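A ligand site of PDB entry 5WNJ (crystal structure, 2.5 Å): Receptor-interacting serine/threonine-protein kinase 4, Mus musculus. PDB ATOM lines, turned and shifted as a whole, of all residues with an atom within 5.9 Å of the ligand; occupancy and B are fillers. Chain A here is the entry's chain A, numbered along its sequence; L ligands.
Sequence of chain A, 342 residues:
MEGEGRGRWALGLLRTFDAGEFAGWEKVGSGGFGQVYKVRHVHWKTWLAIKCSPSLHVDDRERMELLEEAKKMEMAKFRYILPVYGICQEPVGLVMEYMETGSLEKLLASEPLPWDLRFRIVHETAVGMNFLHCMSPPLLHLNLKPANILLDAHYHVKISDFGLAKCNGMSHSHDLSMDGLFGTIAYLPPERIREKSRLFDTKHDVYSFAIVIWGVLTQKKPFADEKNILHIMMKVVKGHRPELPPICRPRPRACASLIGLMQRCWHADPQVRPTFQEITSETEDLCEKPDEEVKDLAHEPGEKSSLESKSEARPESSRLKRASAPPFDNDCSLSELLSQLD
O3 of the ligand sits at hydrogen-bond distance from O of Ala 147, at 2.6 Å.
The backbone NH of Met 99 lies within hydrogen-bond range of an oxygen (O1) of the ligand (2.9 Å).
N1 of the ligand is in hydrogen-bond range of O of Glu 97 (2.9 Å).
O of Val 36 sits at hydrogen-bond distance from N of Gly 29 (3.2 Å).
O of Ala 49 lies within hydrogen-bond range of N of Met 96, 2.7 Å away.
The backbone carbonyl oxygen (O) of Val 36 is in hydrogen-bond range of the backbone NH (N) of Val 28 (2.8 Å).
N of Ser 160 sits at hydrogen-bond distance from O of Asn 148 (3.0 Å).
The side-chain amide nitrogen (ND2) of Asn 148 lies within hydrogen-bond range of the side-chain carboxylate (OD2) of Asp 161, 3.2 Å away.
NZ of Lys 51 is in salt-bridge range of OE1 of Glu 69 (2.8 Å).
Val 28 touches the ligand (CB to C10, 3.7 Å).
Gly 29 touches the ligand.
N of Ser 30 touches C22 of the ligand, 3.8 Å away.
CG2 of Val 36 touches N3 of the ligand, 3.7 Å away.
CB of Ala 49 touches N1 of the ligand, 3.3 Å away.
CD of Lys 51 touches C18 of the ligand (3.7 Å).
CD2 of Leu 82 touches C2 of the ligand, 3.6 Å away.
Met 96 touches the ligand (CE to C16, 3.7 Å).
CA of Tyr 98 touches O1 of the ligand, at 3.4 Å.
Gly 102 touches the ligand (CA to C9, 3.6 Å).
Asn 148 touches the ligand (OD1 to O3, 3.7 Å).
CD1 of Leu 150 touches C3 of the ligand (3.5 Å).
Ser 160 touches the ligand.
Asp 161 touches the ligand.
Of the 24 residues printed, 17 come within 4 Å of the ligand.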
ATOM      1  N   VAL A  28       9.012  14.024  20.479  1.00  0.00           N
ATOM      2  CA  VAL A  28      10.040  13.007  20.778  1.00  0.00           C
ATOM      3  C   VAL A  28      11.450  13.584  21.006  1.00  0.00           C
ATOM      4  O   VAL A  28      12.318  12.880  21.508  1.00  0.00           O
ATOM      5  CB  VAL A  28      10.079  11.900  19.675  1.00  0.00           C
ATOM      6  CG1 VAL A  28       8.745  11.182  19.577  1.00  0.00           C
ATOM      7  CG2 VAL A  28      10.445  12.460  18.303  1.00  0.00           C
ATOM      8  N   GLY A  29      11.671  14.871  20.690  1.00  0.00           N
ATOM      9  CA  GLY A  29      13.018  15.444  20.559  1.00  0.00           C
ATOM     10  C   GLY A  29      13.583  16.174  21.748  1.00  0.00           C
ATOM     11  O   GLY A  29      13.085  16.059  22.876  1.00  0.00           O
ATOM     12  N   SER A  30      14.650  16.938  21.485  1.00  0.00           N
ATOM     13  CA  SER A  30      15.446  17.641  22.513  1.00  0.00           C
ATOM     14  C   SER A  30      15.837  16.758  23.706  1.00  0.00           C
ATOM     15  O   SER A  30      16.215  15.595  23.535  1.00  0.00           O
ATOM     16  CB  SER A  30      14.693  18.888  22.981  1.00  0.00           C
ATOM     17  OG  SER A  30      14.472  19.768  21.894  1.00  0.00           O
ATOM     18  N   GLY A  34      16.156  22.254  18.502  1.00  0.00           N
ATOM     19  CA  GLY A  34      14.973  22.170  17.634  1.00  0.00           C
ATOM     20  C   GLY A  34      14.111  20.985  18.019  1.00  0.00           C
ATOM     21  O   GLY A  34      14.642  19.889  18.250  1.00  0.00           O
ATOM     22  N   VAL A  36      11.600  17.831  17.749  1.00  0.00           N
ATOM     23  CA  VAL A  36      11.255  16.758  16.814  1.00  0.00           C
ATOM     24  C   VAL A  36       9.923  16.140  17.211  1.00  0.00           C
ATOM     25  O   VAL A  36       9.699  15.787  18.391  1.00  0.00           O
ATOM     26  CB  VAL A  36      12.357  15.669  16.723  1.00  0.00           C
ATOM     27  CG1 VAL A  36      11.962  14.575  15.725  1.00  0.00           C
ATOM     28  CG2 VAL A  36      13.671  16.265  16.283  1.00  0.00           C
ATOM     29  N   ALA A  49       8.657  11.957  10.693  1.00  0.00           N
ATOM     30  CA  ALA A  49       9.301  12.747  11.740  1.00  0.00           C
ATOM     31  C   ALA A  49       9.593  14.131  11.186  1.00  0.00           C
ATOM     32  O   ALA A  49      10.075  14.265  10.046  1.00  0.00           O
ATOM     33  CB  ALA A  49      10.599  12.087  12.184  1.00  0.00           C
ATOM     34  N   LYS A  51      11.500  17.822  12.301  1.00  0.00           N
ATOM     35  CA  LYS A  51      12.358  18.595  13.210  1.00  0.00           C
ATOM     36  C   LYS A  51      12.114  20.083  12.926  1.00  0.00           C
ATOM     37  O   LYS A  51      12.549  20.595  11.888  1.00  0.00           O
ATOM     38  CB  LYS A  51      13.830  18.216  12.996  1.00  0.00           C
ATOM     39  CG  LYS A  51      14.829  18.879  13.949  1.00  0.00           C
ATOM     40  CD  LYS A  51      16.268  18.866  13.411  1.00  0.00           C
ATOM     41  CE  LYS A  51      16.404  19.690  12.128  1.00  0.00           C
ATOM     42  NZ  LYS A  51      17.781  20.203  11.879  1.00  0.00           N
ATOM     43  N   GLU A  69      20.584  21.152   4.490  1.00  0.00           N
ATOM     44  CA  GLU A  69      20.548  19.919   5.290  1.00  0.00           C
ATOM     45  C   GLU A  69      19.793  18.806   4.555  1.00  0.00           C
ATOM     46  O   GLU A  69      20.245  17.662   4.524  1.00  0.00           O
ATOM     47  CB  GLU A  69      19.908  20.184   6.666  1.00  0.00           C
ATOM     48  CG  GLU A  69      20.259  19.129   7.709  1.00  0.00           C
ATOM     49  CD  GLU A  69      19.429  19.226   8.984  1.00  0.00           C
ATOM     50  OE1 GLU A  69      18.907  20.324   9.264  1.00  0.00           O
ATOM     51  OE2 GLU A  69      19.306  18.208   9.702  1.00  0.00           O
ATOM     52  N   LEU A  82      19.368   8.003   7.172  1.00  0.00           N
ATOM     53  CA  LEU A  82      17.950   8.356   7.368  1.00  0.00           C
ATOM     54  C   LEU A  82      17.407   9.010   6.105  1.00  0.00           C
ATOM     55  O   LEU A  82      17.975  10.015   5.658  1.00  0.00           O
ATOM     56  CB  LEU A  82      17.766   9.313   8.546  1.00  0.00           C
ATOM     57  CG  LEU A  82      16.306   9.570   8.958  1.00  0.00           C
ATOM     58  CD1 LEU A  82      15.657   8.323   9.557  1.00  0.00           C
ATOM     59  CD2 LEU A  82      16.210  10.727   9.938  1.00  0.00           C
ATOM     60  N   MET A  96      11.133  13.856   7.586  1.00  0.00           N
ATOM     61  CA  MET A  96      12.032  12.692   7.506  1.00  0.00           C
ATOM     62  C   MET A  96      11.314  11.420   7.902  1.00  0.00           C
ATOM     63  O   MET A  96      10.234  11.459   8.497  1.00  0.00           O
ATOM     64  CB  MET A  96      13.211  12.866   8.472  1.00  0.00           C
ATOM     65  CG  MET A  96      14.066  14.103   8.261  1.00  0.00           C
ATOM     66  SD  MET A  96      15.183  14.389   9.647  1.00  0.00           S
ATOM     67  CE  MET A  96      14.047  15.023  10.861  1.00  0.00           C
ATOM     68  N   GLU A  97      11.948  10.280   7.615  1.00  0.00           N
ATOM     69  CA  GLU A  97      11.463   8.979   8.055  1.00  0.00           C
ATOM     70  C   GLU A  97      11.377   8.896   9.585  1.00  0.00           C
ATOM     71  O   GLU A  97      12.205   9.468  10.285  1.00  0.00           O
ATOM     72  CB  GLU A  97      12.357   7.859   7.532  1.00  0.00           C
ATOM     73  CG  GLU A  97      11.785   6.466   7.750  1.00  0.00           C
ATOM     74  CD  GLU A  97      12.515   5.361   7.001  1.00  0.00           C
ATOM     75  OE1 GLU A  97      13.579   4.917   7.481  1.00  0.00           O
ATOM     76  OE2 GLU A  97      12.006   4.918   5.940  1.00  0.00           O
ATOM     77  N   TYR A  98      10.364   8.173  10.069  1.00  0.00           N
ATOM     78  CA  TYR A  98      10.180   7.922  11.501  1.00  0.00           C
ATOM     79  C   TYR A  98      10.845   6.618  11.891  1.00  0.00           C
ATOM     80  O   TYR A  98      10.602   5.592  11.281  1.00  0.00           O
ATOM     81  CB  TYR A  98       8.680   7.856  11.867  1.00  0.00           C
ATOM     82  CG  TYR A  98       8.419   7.579  13.330  1.00  0.00           C
ATOM     83  CD1 TYR A  98       8.900   8.434  14.324  1.00  0.00           C
ATOM     84  CD2 TYR A  98       7.680   6.473  13.736  1.00  0.00           C
ATOM     85  CE1 TYR A  98       8.668   8.177  15.666  1.00  0.00           C
ATOM     86  CE2 TYR A  98       7.439   6.219  15.078  1.00  0.00           C
ATOM     87  CZ  TYR A  98       7.937   7.070  16.043  1.00  0.00           C
ATOM     88  OH  TYR A  98       7.701   6.800  17.370  1.00  0.00           O
ATOM     89  N   MET A  99      11.672   6.678  12.944  1.00  0.00           N
ATOM     90  CA  MET A  99      12.415   5.538  13.453  1.00  0.00           C
ATOM     91  C   MET A  99      11.861   5.176  14.839  1.00  0.00           C
ATOM     92  O   MET A  99      12.243   5.792  15.837  1.00  0.00           O
ATOM     93  CB  MET A  99      13.910   5.903  13.545  1.00  0.00           C
ATOM     94  CG  MET A  99      14.556   6.369  12.247  1.00  0.00           C
ATOM     95  SD  MET A  99      14.712   5.104  10.967  1.00  0.00           S
ATOM     96  CE  MET A  99      15.662   3.854  11.788  1.00  0.00           C
ATOM     97  N   GLU A 100      10.974   4.181  14.889  1.00  0.00           N
ATOM     98  CA  GLU A 100      10.178   3.844  16.087  1.00  0.00           C
ATOM     99  C   GLU A 100      10.971   3.739  17.401  1.00  0.00           C
ATOM    100  O   GLU A 100      10.503   4.196  18.455  1.00  0.00           O
ATOM    101  CB  GLU A 100       9.500   2.488  15.909  1.00  0.00           C
ATOM    102  CG  GLU A 100       8.439   2.407  14.830  1.00  0.00           C
ATOM    103  CD  GLU A 100       7.620   1.130  14.931  1.00  0.00           C
ATOM    104  OE1 GLU A 100       7.422   0.635  16.066  1.00  0.00           O
ATOM    105  OE2 GLU A 100       7.189   0.624  13.878  1.00  0.00           O
ATOM    106  N   THR A 101      12.133   3.107  17.342  1.00  0.00           N
ATOM    107  CA  THR A 101      12.876   2.779  18.552  1.00  0.00           C
ATOM    108  C   THR A 101      13.688   3.959  19.104  1.00  0.00           C
ATOM    109  O   THR A 101      14.144   3.909  20.244  1.00  0.00           O
ATOM    110  CB  THR A 101      13.741   1.514  18.312  1.00  0.00           C
ATOM    111  OG1 THR A 101      12.900   0.462  17.804  1.00  0.00           O
ATOM    112  CG2 THR A 101      14.381   1.039  19.610  1.00  0.00           C
ATOM    113  N   GLY A 102      13.839   5.025  18.324  1.00  0.00           N
ATOM    114  CA  GLY A 102      14.517   6.220  18.806  1.00  0.00           C
ATOM    115  C   GLY A 102      16.026   6.052  18.695  1.00  0.00           C
ATOM    116  O   GLY A 102      16.510   5.373  17.790  1.00  0.00           O
ATOM    117  N   SER A 103      16.761   6.651  19.627  1.00  0.00           N
ATOM    118  CA  SER A 103      18.199   6.785  19.516  1.00  0.00           C
ATOM    119  C   SER A 103      18.955   5.689  20.255  1.00  0.00           C
ATOM    120  O   SER A 103      18.431   5.051  21.169  1.00  0.00           O
ATOM    121  CB  SER A 103      18.634   8.161  20.040  1.00  0.00           C
ATOM    122  OG  SER A 103      18.576   8.223  21.450  1.00  0.00           O
ATOM    123  N   GLU A 105      21.441   6.394  22.153  1.00  0.00           N
ATOM    124  CA  GLU A 105      21.629   6.983  23.484  1.00  0.00           C
ATOM    125  C   GLU A 105      20.575   6.478  24.478  1.00  0.00           C
ATOM    126  O   GLU A 105      20.922   6.069  25.595  1.00  0.00           O
ATOM    127  CB  GLU A 105      21.582   8.507  23.414  1.00  0.00           C
ATOM    128  CG  GLU A 105      21.542   9.164  24.787  1.00  0.00           C
ATOM    129  CD  GLU A 105      21.856  10.641  24.741  1.00  0.00           C
ATOM    130  OE1 GLU A 105      21.212  11.362  23.961  1.00  0.00           O
ATOM    131  OE2 GLU A 105      22.748  11.078  25.515  1.00  0.00           O
ATOM    132  N   ALA A 147      23.191   9.793  20.180  1.00  0.00           N
ATOM    133  CA  ALA A 147      21.957  10.571  19.996  1.00  0.00           C
ATOM    134  C   ALA A 147      21.509  10.730  18.529  1.00  0.00           C
ATOM    135  O   ALA A 147      20.341  10.949  18.273  1.00  0.00           O
ATOM    136  CB  ALA A 147      22.102  11.954  20.646  1.00  0.00           C
ATOM    137  N   ASN A 148      22.441  10.635  17.590  1.00  0.00           N
ATOM    138  CA  ASN A 148      22.167  10.779  16.171  1.00  0.00           C
ATOM    139  C   ASN A 148      22.245   9.456  15.394  1.00  0.00           C
ATOM    140  O   ASN A 148      22.288   9.455  14.165  1.00  0.00           O
ATOM    141  CB  ASN A 148      23.153  11.798  15.572  1.00  0.00           C
ATOM    142  CG  ASN A 148      22.918  13.215  16.091  1.00  0.00           C
ATOM    143  OD1 ASN A 148      21.832  13.552  16.577  1.00  0.00           O
ATOM    144  ND2 ASN A 148      23.947  14.048  15.968  1.00  0.00           N
ATOM    145  N   LEU A 150      19.942   6.409  14.866  1.00  0.00           N
ATOM    146  CA  LEU A 150      18.553   6.025  15.088  1.00  0.00           C
ATOM    147  C   LEU A 150      18.294   4.576  14.716  1.00  0.00           C
ATOM    148  O   LEU A 150      18.995   4.015  13.865  1.00  0.00           O
ATOM    149  CB  LEU A 150      17.629   6.953  14.297  1.00  0.00           C
ATOM    150  CG  LEU A 150      17.780   8.447  14.578  1.00  0.00           C
ATOM    151  CD1 LEU A 150      16.816   9.265  13.718  1.00  0.00           C
ATOM    152  CD2 LEU A 150      17.566   8.741  16.058  1.00  0.00           C
ATOM    153  N   SER A 160      21.376   9.851  11.357  1.00  0.00           N
ATOM    154  CA  SER A 160      20.616  11.096  11.180  1.00  0.00           C
ATOM    155  C   SER A 160      21.434  12.324  11.622  1.00  0.00           C
ATOM    156  O   SER A 160      22.609  12.202  11.968  1.00  0.00           O
ATOM    157  CB  SER A 160      19.256  11.007  11.907  1.00  0.00           C
ATOM    158  OG  SER A 160      19.262  11.666  13.173  1.00  0.00           O
ATOM    159  N   ASP A 161      20.764  13.481  11.592  1.00  0.00           N
ATOM    160  CA  ASP A 161      21.338  14.789  11.935  1.00  0.00           C
ATOM    161  C   ASP A 161      22.500  15.168  11.021  1.00  0.00           C
ATOM    162  O   ASP A 161      23.666  14.969  11.342  1.00  0.00           O
ATOM    163  CB  ASP A 161      21.734  14.882  13.412  1.00  0.00           C
ATOM    164  CG  ASP A 161      21.931  16.348  13.895  1.00  0.00           C
ATOM    165  OD1 ASP A 161      21.766  17.302  13.094  1.00  0.00           O
ATOM    166  OD2 ASP A 161      22.233  16.544  15.092  1.00  0.00           O
ATOM    167  N   PHE A 162      22.159  15.737   9.871  1.00  0.00           N
ATOM    168  CA  PHE A 162      23.140  16.265   8.931  1.00  0.00           C
ATOM    169  C   PHE A 162      23.300  17.794   9.044  1.00  0.00           C
ATOM    170  O   PHE A 162      23.864  18.422   8.142  1.00  0.00           O
ATOM    171  CB  PHE A 162      22.763  15.813   7.517  1.00  0.00           C
ATOM    172  CG  PHE A 162      23.045  14.357   7.262  1.00  0.00           C
ATOM    173  CD1 PHE A 162      22.230  13.371   7.814  1.00  0.00           C
ATOM    174  CD2 PHE A 162      24.153  13.962   6.510  1.00  0.00           C
ATOM    175  CE1 PHE A 162      22.500  12.026   7.601  1.00  0.00           C
ATOM    176  CE2 PHE A 162      24.424  12.624   6.292  1.00  0.00           C
ATOM    177  CZ  PHE A 162      23.591  11.650   6.837  1.00  0.00           C
HETATM  178  O1  LIG L   1      12.182   9.328  13.880  1.00  0.00           O
HETATM  179  C1  LIG L   1      13.030  10.219  13.754  1.00  0.00           C
HETATM  180  N1  LIG L   1      13.571  10.603  12.584  1.00  0.00           N
HETATM  181  C2  LIG L   1      14.296  11.728  12.761  1.00  0.00           C
HETATM  182  C3  LIG L   1      14.541  11.891  14.178  1.00  0.00           C
HETATM  183  C4  LIG L   1      13.687  10.975  14.827  1.00  0.00           C
HETATM  184  C5  LIG L   1      13.703  10.874  16.238  1.00  0.00           C
HETATM  185  C6  LIG L   1      13.026  10.024  17.189  1.00  0.00           C
HETATM  186  C7  LIG L   1      12.081   9.000  17.077  1.00  0.00           C
HETATM  187  C8  LIG L   1      11.644   8.366  18.221  1.00  0.00           C
HETATM  188  C9  LIG L   1      12.120   8.756  19.485  1.00  0.00           C
HETATM  189  C10 LIG L   1      13.051   9.761  19.618  1.00  0.00           C
HETATM  190  C11 LIG L   1      13.502  10.407  18.460  1.00  0.00           C
HETATM  191  N2  LIG L   1      14.404  11.446  18.312  1.00  0.00           N
HETATM  192  C12 LIG L   1      14.541  11.733  16.969  1.00  0.00           C
HETATM  193  C13 LIG L   1      15.365  12.691  16.345  1.00  0.00           C
HETATM  194  C14 LIG L   1      15.364  12.767  14.939  1.00  0.00           C
HETATM  195  C15 LIG L   1      16.276  13.808  14.585  1.00  0.00           C
HETATM  196  C16 LIG L   1      16.699  14.318  13.349  1.00  0.00           C
HETATM  197  C17 LIG L   1      17.627  15.346  13.327  1.00  0.00           C
HETATM  198  C18 LIG L   1      18.148  15.852  14.519  1.00  0.00           C
HETATM  199  C19 LIG L   1      17.733  15.376  15.749  1.00  0.00           C
HETATM  200  C20 LIG L   1      16.804  14.342  15.778  1.00  0.00           C
HETATM  201  N3  LIG L   1      16.225  13.651  16.861  1.00  0.00           N
HETATM  202  C21 LIG L   1      16.412  13.906  18.307  1.00  0.00           C
HETATM  203  C22 LIG L   1      16.563  15.400  18.602  1.00  0.00           C
HETATM  204  O2  LIG L   1      15.213  13.518  18.996  1.00  0.00           O
HETATM  205  C23 LIG L   1      15.215  12.132  19.310  1.00  0.00           C
HETATM  206  C24 LIG L   1      16.687  11.708  19.271  1.00  0.00           C
HETATM  207  C25 LIG L   1      17.468  13.002  18.988  1.00  0.00           C
HETATM  208  O3  LIG L   1      18.505  12.744  18.027  1.00  0.00           O
HETATM  209  C26 LIG L   1      18.097  13.597  20.237  1.00  0.00           C
HETATM  210  O4  LIG L   1      18.850  12.627  20.933  1.00  0.00           O
